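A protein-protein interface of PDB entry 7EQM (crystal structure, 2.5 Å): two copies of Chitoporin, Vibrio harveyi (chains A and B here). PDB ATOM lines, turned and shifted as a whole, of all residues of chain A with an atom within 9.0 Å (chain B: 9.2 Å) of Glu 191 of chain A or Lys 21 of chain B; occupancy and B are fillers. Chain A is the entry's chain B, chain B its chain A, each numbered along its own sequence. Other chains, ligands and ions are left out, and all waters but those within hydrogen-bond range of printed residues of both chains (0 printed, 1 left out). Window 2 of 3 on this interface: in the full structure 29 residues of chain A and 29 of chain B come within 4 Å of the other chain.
No position is printed for both chains.
Printed residues of chain B that touch a printed residue of chain A: Lys 21, Asp 24, Asn 25 and Leu 26.
Hydrophobic or aromatic side chains of chain B that line the printed part of chain A: Leu 26.
Printed residues of chain A that touch a printed residue of chain B: Gly 160, Ala 161, Gly 162, Asp 163 and Glu 191.
Among the printed residues, 8 pairs touch across the chains.
Among the printed residues, Asp or Glu carboxylates within 4 Å of a Lys or Arg side-chain nitrogen of the other chain: Asp 163 of chain A with Lys 21 of chain B (3.7 Å) and Glu 191 of chain A with Lys 21 of chain B (3.0 Å).
Among the printed residues, pairs that only touch across the chains: Gly 160 of chain A with Leu 26 of chain B (3.5 Å), Ala 161 of chain A with Asn 25 of chain B (3.5 Å), Gly 162 of chain A with Asp 24 of chain B (3.6 Å) and Asp 163 of chain A with Asp 24 of chain B (3.8 Å).
The side-chain amino group of Lys 21 of chain B is in salt-bridge range of the side-chain carboxylate of Asp 163 of chain A (3.7 Å).
NZ of Lys 21 of chain B lies within salt-bridge range of OE2 of Glu 191 of chain A.
The side-chain amide oxygen (OD1) of Asn 25 of chain B lies close to the backbone NH (N) of Gly 162 of chain A (3.4 Å).
O of Asn 25 of chain B lies close to O of Gly 160 of chain A (2.9 Å).
The side-chain carboxylate (OD1) of Asp 19 of chain B lies within hydrogen-bond range of the backbone NH (N) of Lys 21 of chain B, at 2.9 Å.
The side-chain amino group (NZ) of Lys 21 of chain B lies within hydrogen-bond range of the side-chain amide oxygen (OD1) of Asn 25 of chain B (2.9 Å).
The backbone carbonyl oxygen (O) of Lys 156 of chain A sits at hydrogen-bond distance from the backbone NH (N) of Ala 161 of chain A (3.0 Å).
The backbone carbonyl oxygen (O) of Asp 163 of chain A lies within hydrogen-bond range of the side-chain amide nitrogen (ND2) of Asn 189 of chain A, at 3.0 Å.
Glu 191 of chain A touches one residue of chain B.
Lys 21 of chain B touches two residues of chain A.
No residue of chain B comes within 4 Å of Ile 190 of chain A.
No residue of chain B comes within 4 Å of Ala 192 of chain A.
Of the printed residues of chain A, Asn 25 of chain B touches Gly 160 (2.9 Å), Ala 161 (3.5 Å) and Gly 162 (3.1 Å).
Of the printed residues of chain B, Gly 162 of chain A touches Asp 24 and Asn 25.
Printed residues of chain A within 4 Å of Asp 24 of chain B: Gly 162 (3.6 Å) and Asp 163 (3.8 Å).
Of the printed residues of chain B, Gly 160 of chain A touches Asn 25 (2.9 Å) and Leu 26 (3.5 Å).
The nearest residue of chain B that does not touch Glu 191 of chain A is Asn 25 of chain B (4.9 Å).
The nearest residue of chain A that does not touch Lys 21 of chain B is Gly 162 of chain A (4.6 Å).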
ATOM      1  N   GLY A 122      -3.859  36.301 -10.446  1.00  0.00           N
ATOM      2  CA  GLY A 122      -3.664  35.057  -9.747  1.00  0.00           C
ATOM      3  C   GLY A 122      -4.802  34.082  -9.991  1.00  0.00           C
ATOM      4  O   GLY A 122      -5.858  34.423 -10.531  1.00  0.00           O
ATOM      5  N   GLY A 123      -4.576  32.837  -9.578  1.00  0.00           N
ATOM      6  CA  GLY A 123      -5.565  31.800  -9.809  1.00  0.00           C
ATOM      7  C   GLY A 123      -5.511  31.340 -11.245  1.00  0.00           C
ATOM      8  O   GLY A 123      -4.439  31.091 -11.778  1.00  0.00           O
ATOM      9  N   ALA A 124      -6.676  31.234 -11.885  1.00  0.00           N
ATOM     10  CA  ALA A 124      -6.772  30.749 -13.263  1.00  0.00           C
ATOM     11  C   ALA A 124      -7.824  31.581 -13.998  1.00  0.00           C
ATOM     12  O   ALA A 124      -9.021  31.325 -13.851  1.00  0.00           O
ATOM     13  CB  ALA A 124      -7.120  29.265 -13.292  1.00  0.00           C
ATOM     14  N   ASP A 155      -7.848  21.376 -13.552  1.00  0.00           N
ATOM     15  CA  ASP A 155      -6.605  20.654 -13.821  1.00  0.00           C
ATOM     16  C   ASP A 155      -6.229  19.712 -12.686  1.00  0.00           C
ATOM     17  O   ASP A 155      -5.848  18.560 -12.924  1.00  0.00           O
ATOM     18  CB  ASP A 155      -5.465  21.631 -14.086  1.00  0.00           C
ATOM     19  CG  ASP A 155      -5.735  22.542 -15.272  1.00  0.00           C
ATOM     20  OD1 ASP A 155      -5.034  23.586 -15.372  1.00  0.00           O
ATOM     21  OD2 ASP A 155      -6.618  22.198 -16.112  1.00  0.00           O
ATOM     22  N   LYS A 156      -6.287  20.187 -11.444  1.00  0.00           N
ATOM     23  CA  LYS A 156      -5.901  19.310 -10.346  1.00  0.00           C
ATOM     24  C   LYS A 156      -6.893  18.163 -10.188  1.00  0.00           C
ATOM     25  O   LYS A 156      -6.492  17.008  -9.994  1.00  0.00           O
ATOM     26  CB  LYS A 156      -5.773  20.112  -9.062  1.00  0.00           C
ATOM     27  CG  LYS A 156      -4.549  21.004  -9.036  1.00  0.00           C
ATOM     28  CD  LYS A 156      -4.039  21.229  -7.610  1.00  0.00           C
ATOM     29  CE  LYS A 156      -2.712  21.983  -7.636  1.00  0.00           C
ATOM     30  NZ  LYS A 156      -1.773  21.475  -8.712  1.00  0.00           N
ATOM     31  N   ALA A 157      -8.191  18.461 -10.304  1.00  0.00           N
ATOM     32  CA  ALA A 157      -9.226  17.438 -10.171  1.00  0.00           C
ATOM     33  C   ALA A 157      -9.098  16.348 -11.226  1.00  0.00           C
ATOM     34  O   ALA A 157      -9.438  15.186 -10.964  1.00  0.00           O
ATOM     35  CB  ALA A 157     -10.605  18.081 -10.262  1.00  0.00           C
ATOM     36  N   GLY A 160      -7.133  13.552  -9.784  1.00  0.00           N
ATOM     37  CA  GLY A 160      -7.460  13.170  -8.415  1.00  0.00           C
ATOM     38  C   GLY A 160      -6.640  13.895  -7.366  1.00  0.00           C
ATOM     39  O   GLY A 160      -6.436  13.372  -6.267  1.00  0.00           O
ATOM     40  N   ALA A 161      -6.157  15.093  -7.684  1.00  0.00           N
ATOM     41  CA  ALA A 161      -5.276  15.861  -6.819  1.00  0.00           C
ATOM     42  C   ALA A 161      -5.911  17.171  -6.366  1.00  0.00           C
ATOM     43  O   ALA A 161      -5.207  18.045  -5.862  1.00  0.00           O
ATOM     44  CB  ALA A 161      -3.959  16.147  -7.546  1.00  0.00           C
ATOM     45  N   GLY A 162      -7.214  17.339  -6.552  1.00  0.00           N
ATOM     46  CA  GLY A 162      -7.877  18.568  -6.160  1.00  0.00           C
ATOM     47  C   GLY A 162      -9.348  18.502  -6.499  1.00  0.00           C
ATOM     48  O   GLY A 162      -9.850  17.498  -7.011  1.00  0.00           O
ATOM     49  N   ASP A 163     -10.043  19.604  -6.198  1.00  0.00           N
ATOM     50  CA  ASP A 163     -11.474  19.731  -6.456  1.00  0.00           C
ATOM     51  C   ASP A 163     -11.776  21.056  -7.146  1.00  0.00           C
ATOM     52  O   ASP A 163     -12.857  21.636  -6.968  1.00  0.00           O
ATOM     53  CB  ASP A 163     -12.289  19.580  -5.165  1.00  0.00           C
ATOM     54  CG  ASP A 163     -11.907  20.598  -4.094  1.00  0.00           C
ATOM     55  OD1 ASP A 163     -10.881  21.302  -4.257  1.00  0.00           O
ATOM     56  OD2 ASP A 163     -12.644  20.695  -3.080  1.00  0.00           O
ATOM     57  N   ASP A 164     -10.823  21.548  -7.933  1.00  0.00           N
ATOM     58  CA  ASP A 164     -11.087  22.710  -8.765  1.00  0.00           C
ATOM     59  C   ASP A 164     -12.124  22.362  -9.837  1.00  0.00           C
ATOM     60  O   ASP A 164     -12.275  21.204 -10.241  1.00  0.00           O
ATOM     61  CB  ASP A 164      -9.785  23.227  -9.393  1.00  0.00           C
ATOM     62  CG  ASP A 164      -8.879  22.102  -9.942  1.00  0.00           C
ATOM     63  OD1 ASP A 164      -9.178  20.906  -9.741  1.00  0.00           O
ATOM     64  OD2 ASP A 164      -7.857  22.417 -10.592  1.00  0.00           O
ATOM     65  N   TYR A 165     -12.879  23.363 -10.263  1.00  0.00           N
ATOM     66  CA  TYR A 165     -13.865  23.179 -11.322  1.00  0.00           C
ATOM     67  C   TYR A 165     -14.134  24.540 -11.950  1.00  0.00           C
ATOM     68  O   TYR A 165     -13.618  25.568 -11.495  1.00  0.00           O
ATOM     69  CB  TYR A 165     -15.152  22.527 -10.801  1.00  0.00           C
ATOM     70  CG  TYR A 165     -15.913  23.349  -9.796  1.00  0.00           C
ATOM     71  CD1 TYR A 165     -15.604  23.292  -8.447  1.00  0.00           C
ATOM     72  CD2 TYR A 165     -16.945  24.173 -10.191  1.00  0.00           C
ATOM     73  CE1 TYR A 165     -16.307  24.039  -7.520  1.00  0.00           C
ATOM     74  CE2 TYR A 165     -17.643  24.922  -9.278  1.00  0.00           C
ATOM     75  CZ  TYR A 165     -17.314  24.858  -7.951  1.00  0.00           C
ATOM     76  OH  TYR A 165     -18.000  25.617  -7.040  1.00  0.00           O
ATOM     77  N   ASN A 187     -13.847  30.146 -12.572  1.00  0.00           N
ATOM     78  CA  ASN A 187     -13.006  29.084 -12.034  1.00  0.00           C
ATOM     79  C   ASN A 187     -13.082  29.081 -10.516  1.00  0.00           C
ATOM     80  O   ASN A 187     -12.933  30.129  -9.874  1.00  0.00           O
ATOM     81  CB  ASN A 187     -11.550  29.238 -12.482  1.00  0.00           C
ATOM     82  CG  ASN A 187     -11.284  28.583 -13.817  1.00  0.00           C
ATOM     83  OD1 ASN A 187     -10.796  27.452 -13.869  1.00  0.00           O
ATOM     84  ND2 ASN A 187     -11.603  29.291 -14.915  1.00  0.00           N
ATOM     85  N   ARG A 188     -13.281  27.898  -9.950  1.00  0.00           N
ATOM     86  CA  ARG A 188     -13.507  27.728  -8.527  1.00  0.00           C
ATOM     87  C   ARG A 188     -12.491  26.753  -7.946  1.00  0.00           C
ATOM     88  O   ARG A 188     -12.027  25.837  -8.631  1.00  0.00           O
ATOM     89  CB  ARG A 188     -14.933  27.230  -8.285  1.00  0.00           C
ATOM     90  CG  ARG A 188     -16.006  28.168  -8.834  1.00  0.00           C
ATOM     91  CD  ARG A 188     -15.941  29.502  -8.119  1.00  0.00           C
ATOM     92  NE  ARG A 188     -16.949  30.458  -8.565  1.00  0.00           N
ATOM     93  CZ  ARG A 188     -16.709  31.421  -9.450  1.00  0.00           C
ATOM     94  NH1 ARG A 188     -15.498  31.542  -9.982  1.00  0.00           N
ATOM     95  NH2 ARG A 188     -17.673  32.263  -9.807  1.00  0.00           N
ATOM     96  N   ASN A 189     -12.147  26.967  -6.672  1.00  0.00           N
ATOM     97  CA  ASN A 189     -11.298  26.063  -5.893  1.00  0.00           C
ATOM     98  C   ASN A 189      -9.881  25.986  -6.456  1.00  0.00           C
ATOM     99  O   ASN A 189      -9.214  24.954  -6.349  1.00  0.00           O
ATOM    100  CB  ASN A 189     -11.913  24.657  -5.787  1.00  0.00           C
ATOM    101  CG  ASN A 189     -13.058  24.574  -4.758  1.00  0.00           C
ATOM    102  OD1 ASN A 189     -13.089  25.316  -3.773  1.00  0.00           O
ATOM    103  ND2 ASN A 189     -13.987  23.653  -4.982  1.00  0.00           N
ATOM    104  N   ILE A 190      -9.409  27.075  -7.056  1.00  0.00           N
ATOM    105  CA  ILE A 190      -8.090  27.102  -7.684  1.00  0.00           C
ATOM    106  C   ILE A 190      -7.038  27.260  -6.595  1.00  0.00           C
ATOM    107  O   ILE A 190      -7.046  28.244  -5.848  1.00  0.00           O
ATOM    108  CB  ILE A 190      -7.986  28.235  -8.716  1.00  0.00           C
ATOM    109  CG1 ILE A 190      -9.083  28.104  -9.790  1.00  0.00           C
ATOM    110  CG2 ILE A 190      -6.590  28.280  -9.327  1.00  0.00           C
ATOM    111  CD1 ILE A 190      -9.055  26.803 -10.600  1.00  0.00           C
ATOM    112  N   GLU A 191      -6.127  26.296  -6.502  1.00  0.00           N
ATOM    113  CA  GLU A 191      -5.082  26.313  -5.486  1.00  0.00           C
ATOM    114  C   GLU A 191      -3.799  26.848  -6.097  1.00  0.00           C
ATOM    115  O   GLU A 191      -3.270  26.260  -7.045  1.00  0.00           O
ATOM    116  CB  GLU A 191      -4.859  24.921  -4.904  1.00  0.00           C
ATOM    117  CG  GLU A 191      -6.008  24.471  -4.022  1.00  0.00           C
ATOM    118  CD  GLU A 191      -5.905  23.010  -3.656  1.00  0.00           C
ATOM    119  OE1 GLU A 191      -4.798  22.437  -3.809  1.00  0.00           O
ATOM    120  OE2 GLU A 191      -6.930  22.436  -3.223  1.00  0.00           O
ATOM    121  N   ALA A 192      -3.303  27.956  -5.547  1.00  0.00           N
ATOM    122  CA  ALA A 192      -2.061  28.560  -6.004  1.00  0.00           C
ATOM    123  C   ALA A 192      -1.566  29.540  -4.950  1.00  0.00           C
ATOM    124  O   ALA A 192      -2.364  30.183  -4.259  1.00  0.00           O
ATOM    125  CB  ALA A 192      -2.245  29.269  -7.352  1.00  0.00           C
ATOM    126  N   GLU A 193      -0.236  29.644  -4.849  1.00  0.00           N
ATOM    127  CA  GLU A 193       0.442  30.593  -3.953  1.00  0.00           C
ATOM    128  C   GLU A 193      -0.054  30.479  -2.510  1.00  0.00           C
ATOM    129  O   GLU A 193      -0.197  31.476  -1.802  1.00  0.00           O
ATOM    130  CB  GLU A 193       0.294  32.032  -4.457  1.00  0.00           C
ATOM    131  CG  GLU A 193       0.672  32.212  -5.911  1.00  0.00           C
ATOM    132  CD  GLU A 193       0.324  33.588  -6.466  1.00  0.00           C
ATOM    133  OE1 GLU A 193      -0.236  34.426  -5.723  1.00  0.00           O
ATOM    134  OE2 GLU A 193       0.627  33.839  -7.658  1.00  0.00           O
ATOM    135  N   GLY A 194      -0.318  29.253  -2.065  1.00  0.00           N
ATOM    136  CA  GLY A 194      -0.793  29.063  -0.712  1.00  0.00           C
ATOM    137  C   GLY A 194      -2.189  29.564  -0.441  1.00  0.00           C
ATOM    138  O   GLY A 194      -2.586  29.641   0.725  1.00  0.00           O
ATOM    139  N   GLN A 195      -2.958  29.901  -1.470  1.00  0.00           N
ATOM    140  CA  GLN A 195      -4.329  30.347  -1.290  1.00  0.00           C
ATOM    141  C   GLN A 195      -5.267  29.504  -2.140  1.00  0.00           C
ATOM    142  O   GLN A 195      -4.846  28.749  -3.020  1.00  0.00           O
ATOM    143  CB  GLN A 195      -4.492  31.829  -1.661  1.00  0.00           C
ATOM    144  CG  GLN A 195      -3.528  32.764  -0.936  1.00  0.00           C
ATOM    145  CD  GLN A 195      -3.751  32.769   0.559  1.00  0.00           C
ATOM    146  OE1 GLN A 195      -4.886  32.857   1.028  1.00  0.00           O
ATOM    147  NE2 GLN A 195      -2.666  32.649   1.319  1.00  0.00           N
ATOM    148  N   THR A 196      -6.558  29.665  -1.885  1.00  0.00           N
ATOM    149  CA  THR A 196      -7.601  29.114  -2.737  1.00  0.00           C
ATOM    150  C   THR A 196      -8.325  30.273  -3.415  1.00  0.00           C
ATOM    151  O   THR A 196      -8.859  31.156  -2.737  1.00  0.00           O
ATOM    152  CB  THR A 196      -8.570  28.245  -1.934  1.00  0.00           C
ATOM    153  OG1 THR A 196      -7.866  27.108  -1.418  1.00  0.00           O
ATOM    154  CG2 THR A 196      -9.692  27.754  -2.823  1.00  0.00           C
ATOM    155  N   TRP A 197      -8.341  30.265  -4.746  1.00  0.00           N
ATOM    156  CA  TRP A 197      -8.812  31.388  -5.541  1.00  0.00           C
ATOM    157  C   TRP A 197     -10.149  31.091  -6.202  1.00  0.00           C
ATOM    158  O   TRP A 197     -10.476  29.937  -6.490  1.00  0.00           O
ATOM    159  CB  TRP A 197      -7.820  31.726  -6.651  1.00  0.00           C
ATOM    160  CG  TRP A 197      -6.465  32.091  -6.222  1.00  0.00           C
ATOM    161  CD1 TRP A 197      -5.468  31.247  -5.814  1.00  0.00           C
ATOM    162  CD2 TRP A 197      -5.917  33.411  -6.199  1.00  0.00           C
ATOM    163  NE1 TRP A 197      -4.339  31.971  -5.516  1.00  0.00           N
ATOM    164  CE2 TRP A 197      -4.589  33.302  -5.754  1.00  0.00           C
ATOM    165  CE3 TRP A 197      -6.430  34.676  -6.496  1.00  0.00           C
ATOM    166  CZ2 TRP A 197      -3.762  34.414  -5.608  1.00  0.00           C
ATOM    167  CZ3 TRP A 197      -5.603  35.781  -6.347  1.00  0.00           C
ATOM    168  CH2 TRP A 197      -4.291  35.642  -5.904  1.00  0.00           C
ATOM    169  N   GLU A 198     -10.896  32.156  -6.487  1.00  0.00           N
ATOM    170  CA  GLU A 198     -12.022  32.121  -7.414  1.00  0.00           C
ATOM    171  C   GLU A 198     -11.811  33.185  -8.484  1.00  0.00           C
ATOM    172  O   GLU A 198     -11.508  34.344  -8.169  1.00  0.00           O
ATOM    173  CB  GLU A 198     -13.344  32.345  -6.697  1.00  0.00           C
ATOM    174  CG  GLU A 198     -13.712  31.195  -5.797  1.00  0.00           C
ATOM    175  CD  GLU A 198     -15.175  31.227  -5.400  1.00  0.00           C
ATOM    176  OE1 GLU A 198     -15.611  30.346  -4.624  1.00  0.00           O
ATOM    177  OE2 GLU A 198     -15.891  32.138  -5.876  1.00  0.00           O
ATOM    178  N   ASN A 199     -11.952  32.791  -9.746  1.00  0.00           N
ATOM    179  CA  ASN A 199     -11.723  33.686 -10.870  1.00  0.00           C
ATOM    180  C   ASN A 199     -13.018  33.912 -11.620  1.00  0.00           C
ATOM    181  O   ASN A 199     -13.819  32.986 -11.780  1.00  0.00           O
ATOM    182  CB  ASN A 199     -10.686  33.129 -11.839  1.00  0.00           C
ATOM    183  CG  ASN A 199      -9.308  33.260 -11.323  1.00  0.00           C
ATOM    184  OD1 ASN A 199      -8.901  32.519 -10.424  1.00  0.00           O
ATOM    185  ND2 ASN A 199      -8.558  34.210 -11.877  1.00  0.00           N
ATOM    186  N   SER A 228      -8.404  33.352  -0.924  1.00  0.00           N
ATOM    187  CA  SER A 228      -9.085  33.012   0.315  1.00  0.00           C
ATOM    188  C   SER A 228      -8.655  33.899   1.475  1.00  0.00           C
ATOM    189  O   SER A 228      -9.425  34.056   2.434  1.00  0.00           O
ATOM    190  CB  SER A 228      -8.867  31.536   0.644  1.00  0.00           C
ATOM    191  OG  SER A 228      -7.510  31.182   0.477  1.00  0.00           O
ATOM    192  N   TYR B  15     -15.090   9.051  -2.056  1.00  0.00           N
ATOM    193  CA  TYR B  15     -14.110   8.341  -1.257  1.00  0.00           C
ATOM    194  C   TYR B  15     -14.379   8.514   0.233  1.00  0.00           C
ATOM    195  O   TYR B  15     -14.973   9.505   0.683  1.00  0.00           O
ATOM    196  CB  TYR B  15     -12.701   8.830  -1.578  1.00  0.00           C
ATOM    197  CG  TYR B  15     -12.061   8.161  -2.776  1.00  0.00           C
ATOM    198  CD1 TYR B  15     -12.375   8.567  -4.076  1.00  0.00           C
ATOM    199  CD2 TYR B  15     -11.122   7.141  -2.605  1.00  0.00           C
ATOM    200  CE1 TYR B  15     -11.787   7.952  -5.176  1.00  0.00           C
ATOM    201  CE2 TYR B  15     -10.525   6.535  -3.681  1.00  0.00           C
ATOM    202  CZ  TYR B  15     -10.861   6.936  -4.966  1.00  0.00           C
ATOM    203  OH  TYR B  15     -10.268   6.320  -6.036  1.00  0.00           O
ATOM    204  N   SER B  17     -11.556   7.886   2.633  1.00  0.00           N
ATOM    205  CA  SER B  17     -10.204   7.483   2.984  1.00  0.00           C
ATOM    206  C   SER B  17      -9.891   7.684   4.457  1.00  0.00           C
ATOM    207  O   SER B  17      -8.919   7.105   4.952  1.00  0.00           O
ATOM    208  CB  SER B  17      -9.190   8.252   2.140  1.00  0.00           C
ATOM    209  OG  SER B  17      -9.385   9.642   2.282  1.00  0.00           O
ATOM    210  N   GLY B  18     -10.696   8.472   5.171  1.00  0.00           N
ATOM    211  CA  GLY B  18     -10.334   8.931   6.493  1.00  0.00           C
ATOM    212  C   GLY B  18      -9.635  10.272   6.512  1.00  0.00           C
ATOM    213  O   GLY B  18      -9.275  10.753   7.598  1.00  0.00           O
ATOM    214  N   ASP B  19      -9.408  10.871   5.341  1.00  0.00           N
ATOM    215  CA  ASP B  19      -8.934  12.243   5.206  1.00  0.00           C
ATOM    216  C   ASP B  19      -9.912  12.994   4.311  1.00  0.00           C
ATOM    217  O   ASP B  19     -10.059  12.654   3.131  1.00  0.00           O
ATOM    218  CB  ASP B  19      -7.525  12.282   4.615  1.00  0.00           C
ATOM    219  CG  ASP B  19      -6.883  13.656   4.714  1.00  0.00           C
ATOM    220  OD1 ASP B  19      -7.590  14.667   4.499  1.00  0.00           O
ATOM    221  OD2 ASP B  19      -5.664  13.721   5.003  1.00  0.00           O
ATOM    222  N   ALA B  20     -10.565  14.024   4.862  1.00  0.00           N
ATOM    223  CA  ALA B  20     -11.587  14.740   4.105  1.00  0.00           C
ATOM    224  C   ALA B  20     -10.995  15.455   2.897  1.00  0.00           C
ATOM    225  O   ALA B  20     -11.646  15.555   1.855  1.00  0.00           O
ATOM    226  CB  ALA B  20     -12.319  15.733   5.005  1.00  0.00           C
ATOM    227  N   LYS B  21      -9.774  15.982   3.021  1.00  0.00           N
ATOM    228  CA  LYS B  21      -9.163  16.680   1.893  1.00  0.00           C
ATOM    229  C   LYS B  21      -8.724  15.698   0.816  1.00  0.00           C
ATOM    230  O   LYS B  21      -8.836  15.985  -0.384  1.00  0.00           O
ATOM    231  CB  LYS B  21      -7.977  17.520   2.363  1.00  0.00           C
ATOM    232  CG  LYS B  21      -7.213  18.202   1.233  1.00  0.00           C
ATOM    233  CD  LYS B  21      -8.135  19.074   0.397  1.00  0.00           C
ATOM    234  CE  LYS B  21      -7.368  19.778  -0.729  1.00  0.00           C
ATOM    235  NZ  LYS B  21      -8.283  20.184  -1.833  1.00  0.00           N
ATOM    236  N   GLN B  22      -8.210  14.539   1.225  1.00  0.00           N
ATOM    237  CA  GLN B  22      -7.955  13.473   0.265  1.00  0.00           C
ATOM    238  C   GLN B  22      -9.248  13.009  -0.406  1.00  0.00           C
ATOM    239  O   GLN B  22      -9.266  12.728  -1.612  1.00  0.00           O
ATOM    240  CB  GLN B  22      -7.251  12.310   0.964  1.00  0.00           C
ATOM    241  CG  GLN B  22      -7.159  11.065   0.108  1.00  0.00           C
ATOM    242  CD  GLN B  22      -6.270  10.015   0.713  1.00  0.00           C
ATOM    243  OE1 GLN B  22      -5.394  10.322   1.528  1.00  0.00           O
ATOM    244  NE2 GLN B  22      -6.481   8.763   0.316  1.00  0.00           N
ATOM    245  N   ASP B  23     -10.342  12.919   0.360  1.00  0.00           N
ATOM    246  CA  ASP B  23     -11.620  12.528  -0.227  1.00  0.00           C
ATOM    247  C   ASP B  23     -12.057  13.534  -1.272  1.00  0.00           C
ATOM    248  O   ASP B  23     -12.514  13.159  -2.359  1.00  0.00           O
ATOM    249  CB  ASP B  23     -12.692  12.401   0.850  1.00  0.00           C
ATOM    250  CG  ASP B  23     -12.433  11.256   1.810  1.00  0.00           C
ATOM    251  OD1 ASP B  23     -11.537  10.421   1.528  1.00  0.00           O
ATOM    252  OD2 ASP B  23     -13.134  11.196   2.852  1.00  0.00           O
ATOM    253  N   ASP B  24     -11.922  14.819  -0.956  1.00  0.00           N
ATOM    254  CA  ASP B  24     -12.208  15.852  -1.941  1.00  0.00           C
ATOM    255  C   ASP B  24     -11.284  15.733  -3.153  1.00  0.00           C
ATOM    256  O   ASP B  24     -11.712  15.957  -4.291  1.00  0.00           O
ATOM    257  CB  ASP B  24     -12.080  17.233  -1.296  1.00  0.00           C
ATOM    258  CG  ASP B  24     -13.156  17.507  -0.243  1.00  0.00           C
ATOM    259  OD1 ASP B  24     -14.264  16.902  -0.307  1.00  0.00           O
ATOM    260  OD2 ASP B  24     -12.881  18.354   0.644  1.00  0.00           O
ATOM    261  N   ASN B  25     -10.020  15.360  -2.929  1.00  0.00           N
ATOM    262  CA  ASN B  25      -9.032  15.319  -4.003  1.00  0.00           C
ATOM    263  C   ASN B  25      -9.231  14.125  -4.923  1.00  0.00           C
ATOM    264  O   ASN B  25      -9.233  14.272  -6.152  1.00  0.00           O
ATOM    265  CB  ASN B  25      -7.626  15.264  -3.424  1.00  0.00           C
ATOM    266  CG  ASN B  25      -7.153  16.597  -2.944  1.00  0.00           C
ATOM    267  OD1 ASN B  25      -7.789  17.633  -3.198  1.00  0.00           O
ATOM    268  ND2 ASN B  25      -6.032  16.593  -2.237  1.00  0.00           N
ATOM    269  N   LEU B  26      -9.349  12.928  -4.340  1.00  0.00           N
ATOM    270  CA  LEU B  26      -9.489  11.724  -5.144  1.00  0.00           C
ATOM    271  C   LEU B  26     -10.875  11.627  -5.748  1.00  0.00           C
ATOM    272  O   LEU B  26     -11.033  11.092  -6.850  1.00  0.00           O
ATOM    273  CB  LEU B  26      -9.187  10.484  -4.295  1.00  0.00           C
ATOM    274  CG  LEU B  26      -7.698  10.168  -4.076  1.00  0.00           C
ATOM    275  CD1 LEU B  26      -7.538   9.096  -3.025  1.00  0.00           C
ATOM    276  CD2 LEU B  26      -6.989   9.739  -5.370  1.00  0.00           C
ATOM    277  N   GLY B  27     -11.890  12.123  -5.044  1.00  0.00           N
ATOM    278  CA  GLY B  27     -13.265  11.946  -5.460  1.00  0.00           C
ATOM    279  C   GLY B  27     -13.794  13.121  -6.268  1.00  0.00           C
ATOM    280  O   GLY B  27     -13.107  14.099  -6.552  1.00  0.00           O
